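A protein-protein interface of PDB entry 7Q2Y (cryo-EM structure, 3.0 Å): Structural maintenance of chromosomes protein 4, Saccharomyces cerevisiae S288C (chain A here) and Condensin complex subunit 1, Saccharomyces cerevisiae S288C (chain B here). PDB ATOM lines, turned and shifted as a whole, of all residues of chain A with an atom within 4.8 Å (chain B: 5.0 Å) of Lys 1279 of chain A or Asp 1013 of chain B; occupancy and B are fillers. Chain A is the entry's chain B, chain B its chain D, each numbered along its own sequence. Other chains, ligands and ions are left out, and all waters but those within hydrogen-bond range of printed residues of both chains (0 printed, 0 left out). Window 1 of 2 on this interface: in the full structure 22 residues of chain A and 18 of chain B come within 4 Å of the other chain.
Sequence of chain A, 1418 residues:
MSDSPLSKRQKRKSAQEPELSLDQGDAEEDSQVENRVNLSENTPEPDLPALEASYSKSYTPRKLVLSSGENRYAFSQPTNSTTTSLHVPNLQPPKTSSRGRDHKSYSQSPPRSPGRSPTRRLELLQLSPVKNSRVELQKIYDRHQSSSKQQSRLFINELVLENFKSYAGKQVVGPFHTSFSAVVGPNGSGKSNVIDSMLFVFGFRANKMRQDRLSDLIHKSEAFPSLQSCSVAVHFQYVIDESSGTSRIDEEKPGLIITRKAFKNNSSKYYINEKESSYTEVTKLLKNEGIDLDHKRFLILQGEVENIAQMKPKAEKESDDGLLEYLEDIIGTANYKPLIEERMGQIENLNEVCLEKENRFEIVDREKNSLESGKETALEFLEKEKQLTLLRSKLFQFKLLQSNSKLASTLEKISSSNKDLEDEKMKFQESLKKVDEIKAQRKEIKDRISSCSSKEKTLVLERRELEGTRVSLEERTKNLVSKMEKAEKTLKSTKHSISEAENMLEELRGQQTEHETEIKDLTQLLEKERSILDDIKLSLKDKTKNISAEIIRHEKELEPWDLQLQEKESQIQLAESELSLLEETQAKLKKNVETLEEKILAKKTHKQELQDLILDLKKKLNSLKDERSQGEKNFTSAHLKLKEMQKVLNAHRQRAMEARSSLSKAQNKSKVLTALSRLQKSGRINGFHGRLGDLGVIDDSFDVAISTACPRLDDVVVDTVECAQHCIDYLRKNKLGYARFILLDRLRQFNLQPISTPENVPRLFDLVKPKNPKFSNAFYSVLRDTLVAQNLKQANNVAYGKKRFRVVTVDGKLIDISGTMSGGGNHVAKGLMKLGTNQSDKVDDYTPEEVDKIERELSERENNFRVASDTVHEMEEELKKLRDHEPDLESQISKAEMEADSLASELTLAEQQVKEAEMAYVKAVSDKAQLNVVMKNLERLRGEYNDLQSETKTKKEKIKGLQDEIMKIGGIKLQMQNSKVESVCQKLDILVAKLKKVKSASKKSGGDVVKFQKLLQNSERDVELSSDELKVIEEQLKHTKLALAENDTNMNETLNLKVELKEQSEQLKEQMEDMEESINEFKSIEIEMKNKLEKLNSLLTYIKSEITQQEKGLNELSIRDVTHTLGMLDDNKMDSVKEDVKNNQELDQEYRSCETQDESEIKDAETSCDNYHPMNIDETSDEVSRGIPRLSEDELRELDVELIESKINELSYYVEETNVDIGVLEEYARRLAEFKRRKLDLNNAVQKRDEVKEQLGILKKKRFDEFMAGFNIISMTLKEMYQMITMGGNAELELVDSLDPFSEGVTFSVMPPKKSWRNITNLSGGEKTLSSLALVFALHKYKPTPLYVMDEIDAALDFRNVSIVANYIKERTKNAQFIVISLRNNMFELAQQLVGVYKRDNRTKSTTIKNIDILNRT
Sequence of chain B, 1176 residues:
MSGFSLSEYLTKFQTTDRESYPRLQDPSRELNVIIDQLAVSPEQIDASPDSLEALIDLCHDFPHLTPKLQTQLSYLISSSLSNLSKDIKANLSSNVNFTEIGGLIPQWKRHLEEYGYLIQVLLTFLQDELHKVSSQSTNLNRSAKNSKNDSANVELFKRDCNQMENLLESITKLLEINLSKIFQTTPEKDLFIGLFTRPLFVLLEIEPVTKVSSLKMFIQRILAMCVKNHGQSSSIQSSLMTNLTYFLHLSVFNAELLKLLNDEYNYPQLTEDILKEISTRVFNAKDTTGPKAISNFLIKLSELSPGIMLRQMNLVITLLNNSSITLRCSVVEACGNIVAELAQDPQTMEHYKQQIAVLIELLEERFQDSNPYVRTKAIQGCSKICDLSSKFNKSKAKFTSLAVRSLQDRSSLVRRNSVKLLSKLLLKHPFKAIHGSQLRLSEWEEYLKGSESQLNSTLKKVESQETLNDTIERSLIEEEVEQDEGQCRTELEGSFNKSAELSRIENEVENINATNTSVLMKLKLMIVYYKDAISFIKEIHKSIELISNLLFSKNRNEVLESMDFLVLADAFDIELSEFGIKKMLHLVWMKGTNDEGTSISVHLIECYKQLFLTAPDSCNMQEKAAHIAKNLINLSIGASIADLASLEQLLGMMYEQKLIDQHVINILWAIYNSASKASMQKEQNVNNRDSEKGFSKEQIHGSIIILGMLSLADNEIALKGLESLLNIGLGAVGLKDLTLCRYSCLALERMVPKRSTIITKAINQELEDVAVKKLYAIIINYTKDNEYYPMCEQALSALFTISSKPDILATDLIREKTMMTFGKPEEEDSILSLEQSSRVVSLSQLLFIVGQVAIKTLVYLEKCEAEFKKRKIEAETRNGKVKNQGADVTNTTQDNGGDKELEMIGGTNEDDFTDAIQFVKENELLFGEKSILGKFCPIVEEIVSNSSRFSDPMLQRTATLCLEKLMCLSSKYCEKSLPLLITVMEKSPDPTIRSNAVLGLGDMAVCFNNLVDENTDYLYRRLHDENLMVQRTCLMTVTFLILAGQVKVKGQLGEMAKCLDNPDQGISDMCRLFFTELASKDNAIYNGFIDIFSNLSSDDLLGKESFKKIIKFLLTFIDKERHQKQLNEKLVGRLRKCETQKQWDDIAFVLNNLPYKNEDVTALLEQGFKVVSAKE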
ATOM      1  N   SER A 133     -16.442 -29.886  14.503  1.00  0.00           N
ATOM      2  CA  SER A 133     -17.644 -29.344  15.131  1.00  0.00           C
ATOM      3  C   SER A 133     -18.196 -30.243  16.230  1.00  0.00           C
ATOM      4  O   SER A 133     -19.236 -29.913  16.813  1.00  0.00           O
ATOM      5  CB  SER A 133     -18.762 -29.051  14.117  1.00  0.00           C
ATOM      6  OG  SER A 133     -19.888 -28.472  14.753  1.00  0.00           O
ATOM      7  N   SER A1275     -24.860 -22.090  17.144  1.00  0.00           N
ATOM      8  CA  SER A1275     -24.945 -22.751  15.846  1.00  0.00           C
ATOM      9  C   SER A1275     -24.476 -24.196  15.935  1.00  0.00           C
ATOM     10  O   SER A1275     -25.126 -25.106  15.402  1.00  0.00           O
ATOM     11  CB  SER A1275     -24.125 -21.979  14.812  1.00  0.00           C
ATOM     12  OG  SER A1275     -22.740 -22.050  15.105  1.00  0.00           O
ATOM     13  N   MET A1276     -23.350 -24.432  16.616  1.00  0.00           N
ATOM     14  CA  MET A1276     -22.892 -25.808  16.794  1.00  0.00           C
ATOM     15  C   MET A1276     -23.906 -26.624  17.589  1.00  0.00           C
ATOM     16  O   MET A1276     -24.218 -27.772  17.231  1.00  0.00           O
ATOM     17  CB  MET A1276     -21.527 -25.824  17.483  1.00  0.00           C
ATOM     18  CG  MET A1276     -20.402 -25.232  16.648  1.00  0.00           C
ATOM     19  SD  MET A1276     -18.799 -25.328  17.468  1.00  0.00           S
ATOM     20  CE  MET A1276     -18.975 -24.050  18.711  1.00  0.00           C
ATOM     21  N   THR A1277     -24.447 -26.037  18.661  1.00  0.00           N
ATOM     22  CA  THR A1277     -25.423 -26.743  19.482  1.00  0.00           C
ATOM     23  C   THR A1277     -26.678 -27.074  18.687  1.00  0.00           C
ATOM     24  O   THR A1277     -27.227 -28.170  18.816  1.00  0.00           O
ATOM     25  CB  THR A1277     -25.774 -25.908  20.714  1.00  0.00           C
ATOM     26  OG1 THR A1277     -24.569 -25.460  21.346  1.00  0.00           O
ATOM     27  CG2 THR A1277     -26.577 -26.736  21.704  1.00  0.00           C
ATOM     28  N   LEU A1278     -27.141 -26.141  17.851  1.00  0.00           N
ATOM     29  CA  LEU A1278     -28.346 -26.375  17.062  1.00  0.00           C
ATOM     30  C   LEU A1278     -28.111 -27.429  15.990  1.00  0.00           C
ATOM     31  O   LEU A1278     -28.995 -28.251  15.722  1.00  0.00           O
ATOM     32  CB  LEU A1278     -28.823 -25.066  16.433  1.00  0.00           C
ATOM     33  CG  LEU A1278     -29.827 -25.189  15.286  1.00  0.00           C
ATOM     34  CD1 LEU A1278     -31.137 -25.789  15.771  1.00  0.00           C
ATOM     35  CD2 LEU A1278     -30.066 -23.840  14.638  1.00  0.00           C
ATOM     36  N   LYS A1279     -26.937 -27.418  15.356  1.00  0.00           N
ATOM     37  CA  LYS A1279     -26.633 -28.460  14.380  1.00  0.00           C
ATOM     38  C   LYS A1279     -26.648 -29.836  15.032  1.00  0.00           C
ATOM     39  O   LYS A1279     -27.296 -30.766  14.529  1.00  0.00           O
ATOM     40  CB  LYS A1279     -25.280 -28.188  13.724  1.00  0.00           C
ATOM     41  CG  LYS A1279     -24.938 -29.139  12.591  1.00  0.00           C
ATOM     42  CD  LYS A1279     -23.586 -28.806  11.984  1.00  0.00           C
ATOM     43  CE  LYS A1279     -23.642 -27.511  11.191  1.00  0.00           C
ATOM     44  NZ  LYS A1279     -24.494 -27.636   9.976  1.00  0.00           N
ATOM     45  N   GLU A1280     -25.970 -29.974  16.177  1.00  0.00           N
ATOM     46  CA  GLU A1280     -25.980 -31.252  16.884  1.00  0.00           C
ATOM     47  C   GLU A1280     -27.388 -31.623  17.337  1.00  0.00           C
ATOM     48  O   GLU A1280     -27.783 -32.794  17.271  1.00  0.00           O
ATOM     49  CB  GLU A1280     -25.026 -31.197  18.080  1.00  0.00           C
ATOM     50  CG  GLU A1280     -24.662 -32.543  18.745  1.00  0.00           C
ATOM     51  CD  GLU A1280     -24.201 -33.657  17.796  1.00  0.00           C
ATOM     52  OE1 GLU A1280     -24.092 -33.451  16.569  1.00  0.00           O
ATOM     53  OE2 GLU A1280     -23.942 -34.772  18.300  1.00  0.00           O
ATOM     54  N   MET A1281     -28.161 -30.634  17.792  1.00  0.00           N
ATOM     55  CA  MET A1281     -29.503 -30.890  18.297  1.00  0.00           C
ATOM     56  C   MET A1281     -30.420 -31.398  17.194  1.00  0.00           C
ATOM     57  O   MET A1281     -31.177 -32.351  17.399  1.00  0.00           O
ATOM     58  CB  MET A1281     -30.069 -29.610  18.908  1.00  0.00           C
ATOM     59  CG  MET A1281     -31.409 -29.776  19.583  1.00  0.00           C
ATOM     60  SD  MET A1281     -31.220 -30.889  20.980  1.00  0.00           S
ATOM     61  CE  MET A1281     -30.321 -29.806  22.085  1.00  0.00           C
ATOM     62  N   TYR A1282     -30.372 -30.764  16.021  1.00  0.00           N
ATOM     63  CA  TYR A1282     -31.188 -31.217  14.901  1.00  0.00           C
ATOM     64  C   TYR A1282     -30.741 -32.591  14.424  1.00  0.00           C
ATOM     65  O   TYR A1282     -31.576 -33.442  14.092  1.00  0.00           O
ATOM     66  CB  TYR A1282     -31.130 -30.204  13.759  1.00  0.00           C
ATOM     67  CG  TYR A1282     -32.282 -30.318  12.788  1.00  0.00           C
ATOM     68  CD1 TYR A1282     -33.563 -29.924  13.150  1.00  0.00           C
ATOM     69  CD2 TYR A1282     -32.092 -30.828  11.510  1.00  0.00           C
ATOM     70  CE1 TYR A1282     -34.619 -30.027  12.269  1.00  0.00           C
ATOM     71  CE2 TYR A1282     -33.144 -30.937  10.621  1.00  0.00           C
ATOM     72  CZ  TYR A1282     -34.405 -30.536  11.006  1.00  0.00           C
ATOM     73  OH  TYR A1282     -35.457 -30.643  10.125  1.00  0.00           O
ATOM     74  N   GLN A1283     -29.425 -32.833  14.398  1.00  0.00           N
ATOM     75  CA  GLN A1283     -28.930 -34.153  14.027  1.00  0.00           C
ATOM     76  C   GLN A1283     -29.456 -35.226  14.972  1.00  0.00           C
ATOM     77  O   GLN A1283     -29.826 -36.322  14.538  1.00  0.00           O
ATOM     78  CB  GLN A1283     -27.401 -34.155  14.019  1.00  0.00           C
ATOM     79  CG  GLN A1283     -26.775 -35.057  12.969  1.00  0.00           C
ATOM     80  CD  GLN A1283     -25.261 -35.072  13.047  1.00  0.00           C
ATOM     81  OE1 GLN A1283     -24.641 -34.099  13.478  1.00  0.00           O
ATOM     82  NE2 GLN A1283     -24.656 -36.182  12.641  1.00  0.00           N
ATOM     83  N   ASN A1290     -29.534 -31.411   8.680  1.00  0.00           N
ATOM     84  CA  ASN A1290     -28.659 -30.358   9.174  1.00  0.00           C
ATOM     85  C   ASN A1290     -29.481 -29.128   9.522  1.00  0.00           C
ATOM     86  O   ASN A1290     -30.553 -28.897   8.959  1.00  0.00           O
ATOM     87  CB  ASN A1290     -27.584 -29.981   8.144  1.00  0.00           C
ATOM     88  CG  ASN A1290     -26.574 -31.088   7.920  1.00  0.00           C
ATOM     89  OD1 ASN A1290     -26.926 -32.194   7.510  1.00  0.00           O
ATOM     90  ND2 ASN A1290     -25.307 -30.794   8.188  1.00  0.00           N
ATOM     91  N   ALA A1291     -28.964 -28.336  10.457  1.00  0.00           N
ATOM     92  CA  ALA A1291     -29.559 -27.053  10.814  1.00  0.00           C
ATOM     93  C   ALA A1291     -28.435 -26.041  10.951  1.00  0.00           C
ATOM     94  O   ALA A1291     -27.562 -26.199  11.811  1.00  0.00           O
ATOM     95  CB  ALA A1291     -30.363 -27.150  12.112  1.00  0.00           C
ATOM     96  N   GLU A1292     -28.451 -25.009  10.112  1.00  0.00           N
ATOM     97  CA  GLU A1292     -27.370 -24.036  10.073  1.00  0.00           C
ATOM     98  C   GLU A1292     -27.926 -22.630  10.229  1.00  0.00           C
ATOM     99  O   GLU A1292     -28.872 -22.249   9.532  1.00  0.00           O
ATOM    100  CB  GLU A1292     -26.577 -24.148   8.767  1.00  0.00           C
ATOM    101  CG  GLU A1292     -25.381 -23.215   8.687  1.00  0.00           C
ATOM    102  CD  GLU A1292     -24.593 -23.390   7.404  1.00  0.00           C
ATOM    103  OE1 GLU A1292     -24.995 -24.226   6.567  1.00  0.00           O
ATOM    104  OE2 GLU A1292     -23.571 -22.691   7.231  1.00  0.00           O
ATOM    105  N   TRP A1317     -31.319 -29.430   0.722  1.00  0.00           N
ATOM    106  CA  TRP A1317     -31.559 -28.184   1.438  1.00  0.00           C
ATOM    107  C   TRP A1317     -32.792 -27.485   0.880  1.00  0.00           C
ATOM    108  O   TRP A1317     -32.927 -27.313  -0.335  1.00  0.00           O
ATOM    109  CB  TRP A1317     -30.340 -27.267   1.336  1.00  0.00           C
ATOM    110  CG  TRP A1317     -29.178 -27.709   2.170  1.00  0.00           C
ATOM    111  CD1 TRP A1317     -28.178 -28.558   1.798  1.00  0.00           C
ATOM    112  CD2 TRP A1317     -28.897 -27.327   3.521  1.00  0.00           C
ATOM    113  NE1 TRP A1317     -27.291 -28.726   2.832  1.00  0.00           N
ATOM    114  CE2 TRP A1317     -27.710 -27.981   3.902  1.00  0.00           C
ATOM    115  CE3 TRP A1317     -29.534 -26.494   4.447  1.00  0.00           C
ATOM    116  CZ2 TRP A1317     -27.147 -27.830   5.166  1.00  0.00           C
ATOM    117  CZ3 TRP A1317     -28.972 -26.345   5.701  1.00  0.00           C
ATOM    118  CH2 TRP A1317     -27.792 -27.009   6.049  1.00  0.00           C
ATOM    119  N   ASN B1009     -22.887 -36.081   5.121  1.00  0.00           N
ATOM    120  CA  ASN B1009     -22.700 -34.648   4.926  1.00  0.00           C
ATOM    121  C   ASN B1009     -22.531 -33.907   6.247  1.00  0.00           C
ATOM    122  O   ASN B1009     -22.083 -32.755   6.252  1.00  0.00           O
ATOM    123  CB  ASN B1009     -23.888 -34.076   4.147  1.00  0.00           C
ATOM    124  CG  ASN B1009     -23.597 -32.715   3.539  1.00  0.00           C
ATOM    125  OD1 ASN B1009     -22.488 -32.193   3.647  1.00  0.00           O
ATOM    126  ND2 ASN B1009     -24.600 -32.133   2.892  1.00  0.00           N
ATOM    127  N   ASN B1010     -22.882 -34.542   7.368  1.00  0.00           N
ATOM    128  CA  ASN B1010     -22.833 -33.863   8.659  1.00  0.00           C
ATOM    129  C   ASN B1010     -21.415 -33.450   9.034  1.00  0.00           C
ATOM    130  O   ASN B1010     -21.223 -32.416   9.684  1.00  0.00           O
ATOM    131  CB  ASN B1010     -23.429 -34.765   9.740  1.00  0.00           C
ATOM    132  CG  ASN B1010     -24.928 -34.933   9.593  1.00  0.00           C
ATOM    133  OD1 ASN B1010     -25.646 -33.974   9.309  1.00  0.00           O
ATOM    134  ND2 ASN B1010     -25.408 -36.157   9.775  1.00  0.00           N
ATOM    135  N   LEU B1011     -20.416 -34.238   8.641  1.00  0.00           N
ATOM    136  CA  LEU B1011     -19.029 -33.956   8.987  1.00  0.00           C
ATOM    137  C   LEU B1011     -18.277 -33.185   7.909  1.00  0.00           C
ATOM    138  O   LEU B1011     -17.086 -32.909   8.089  1.00  0.00           O
ATOM    139  CB  LEU B1011     -18.297 -35.270   9.303  1.00  0.00           C
ATOM    140  CG  LEU B1011     -18.163 -36.360   8.230  1.00  0.00           C
ATOM    141  CD1 LEU B1011     -16.991 -36.121   7.280  1.00  0.00           C
ATOM    142  CD2 LEU B1011     -18.054 -37.732   8.880  1.00  0.00           C
ATOM    143  N   VAL B1012     -18.930 -32.832   6.800  1.00  0.00           N
ATOM    144  CA  VAL B1012     -18.257 -32.205   5.670  1.00  0.00           C
ATOM    145  C   VAL B1012     -18.978 -30.961   5.171  1.00  0.00           C
ATOM    146  O   VAL B1012     -18.466 -30.276   4.281  1.00  0.00           O
ATOM    147  CB  VAL B1012     -18.071 -33.217   4.520  1.00  0.00           C
ATOM    148  CG1 VAL B1012     -19.396 -33.479   3.840  1.00  0.00           C
ATOM    149  CG2 VAL B1012     -16.990 -32.770   3.532  1.00  0.00           C
ATOM    150  N   ASP B1013     -20.158 -30.640   5.710  1.00  0.00           N
ATOM    151  CA  ASP B1013     -20.828 -29.403   5.319  1.00  0.00           C
ATOM    152  C   ASP B1013     -19.945 -28.183   5.553  1.00  0.00           C
ATOM    153  O   ASP B1013     -20.044 -27.195   4.816  1.00  0.00           O
ATOM    154  CB  ASP B1013     -22.145 -29.257   6.083  1.00  0.00           C
ATOM    155  CG  ASP B1013     -23.086 -28.257   5.442  1.00  0.00           C
ATOM    156  OD1 ASP B1013     -22.769 -27.755   4.343  1.00  0.00           O
ATOM    157  OD2 ASP B1013     -24.143 -27.968   6.041  1.00  0.00           O
ATOM    158  N   GLU B1014     -19.078 -28.231   6.564  1.00  0.00           N
ATOM    159  CA  GLU B1014     -18.159 -27.136   6.835  1.00  0.00           C
ATOM    160  C   GLU B1014     -16.809 -27.303   6.149  1.00  0.00           C
ATOM    161  O   GLU B1014     -16.111 -26.304   5.939  1.00  0.00           O
ATOM    162  CB  GLU B1014     -17.946 -26.990   8.345  1.00  0.00           C
ATOM    163  CG  GLU B1014     -17.428 -28.247   9.023  1.00  0.00           C
ATOM    164  CD  GLU B1014     -18.542 -29.127   9.559  1.00  0.00           C
ATOM    165  OE1 GLU B1014     -19.593 -29.233   8.892  1.00  0.00           O
ATOM    166  OE2 GLU B1014     -18.367 -29.714  10.646  1.00  0.00           O
ATOM    167  N   ASN B1015     -16.426 -28.528   5.796  1.00  0.00           N
ATOM    168  CA  ASN B1015     -15.147 -28.789   5.149  1.00  0.00           C
ATOM    169  C   ASN B1015     -15.222 -28.724   3.628  1.00  0.00           C
ATOM    170  O   ASN B1015     -14.182 -28.807   2.968  1.00  0.00           O
ATOM    171  CB  ASN B1015     -14.609 -30.158   5.578  1.00  0.00           C
ATOM    172  CG  ASN B1015     -14.088 -30.155   7.001  1.00  0.00           C
ATOM    173  OD1 ASN B1015     -13.406 -29.222   7.423  1.00  0.00           O
ATOM    174  ND2 ASN B1015     -14.409 -31.203   7.751  1.00  0.00           N
ATOM    175  N   THR B1016     -16.424 -28.590   3.061  1.00  0.00           N
ATOM    176  CA  THR B1016     -16.559 -28.417   1.615  1.00  0.00           C
ATOM    177  C   THR B1016     -15.832 -27.185   1.082  1.00  0.00           C
ATOM    178  O   THR B1016     -15.782 -27.000  -0.141  1.00  0.00           O
ATOM    179  CB  THR B1016     -18.037 -28.335   1.220  1.00  0.00           C
ATOM    180  OG1 THR B1016     -18.737 -27.486   2.140  1.00  0.00           O
ATOM    181  CG2 THR B1016     -18.673 -29.717   1.204  1.00  0.00           C
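The side-chain amino group (NZ) of Lys 1279 of chain A lies within salt-bridge range of the side-chain carboxylate (OD2) of Asp 1013 of chain B (3.96 Å). The side-chain amide nitrogen (NE2) of Gln 1283 of chain A lies close to the side-chain amide nitrogen (ND2) of Asn 1010 of chain B (3.0 Å). The side-chain amide oxygen (OD1) of Asn 1010 of chain B sits close to the side-chain amide oxygen (OD1) of Asn 1290 of chain A, at 2.8 Å.
OE2 of Glu 1014 of chain B touches CB of Ser 133 of chain A, at 3.6 Å. OD2 of Asp 1013 of chain B touches ND2 of Asn 1290 of chain A (3.7 Å). Glu 1292 of chain A touches Asp 1013 of chain B (OE1 to OD2, 3.9 Å). CZ2 of Trp 1317 of chain A touches OD2 of Asp 1013 of chain B (3.1 Å).
Printed residues of chain B within 4 Å of Lys 1279 of chain A: Asp 1013. Of the printed residues of chain A, Asn 1010 of chain B touches Gln 1283 (3.0 Å) and Asn 1290 (2.8 Å). Of the printed residues of chain B, Gln 1283 of chain A touches Asn 1010. Ala 1291 of chain A touches none of the printed residues of chain B. Thr 1016 of chain B touches none of the printed residues of chain A. The nearest residue of chain B that does not touch Lys 1279 of chain A is Asn 1010 of chain B (4.9 Å). The nearest printed residue of chain A that does not touch Asn 1010 of chain B is Lys 1279 of chain A (4.9 Å).
The side-chain carboxylate of Glu 1280 of chain A sits close to the side-chain amide oxygen of Gln 1283 of chain A (3.2 Å). OD1 of Asn 1009 of chain B is in hydrogen-bond range of N of Asp 1013 of chain B. The backbone carbonyl oxygen of Asp 1013 of chain B sits at hydrogen-bond distance from the side-chain hydroxyl of Thr 1016 of chain B, at 3.0 Å.
Of the 8 printed residues of chain B, 3 touch a printed residue of chain A. Of the 14 printed residues of chain A, 6 touch a printed residue of chain B. Hydrophobic or aromatic side chains of chain A that line the printed part of chain B: Trp 1317. Among the printed residues, 7 pairs touch across the chains.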
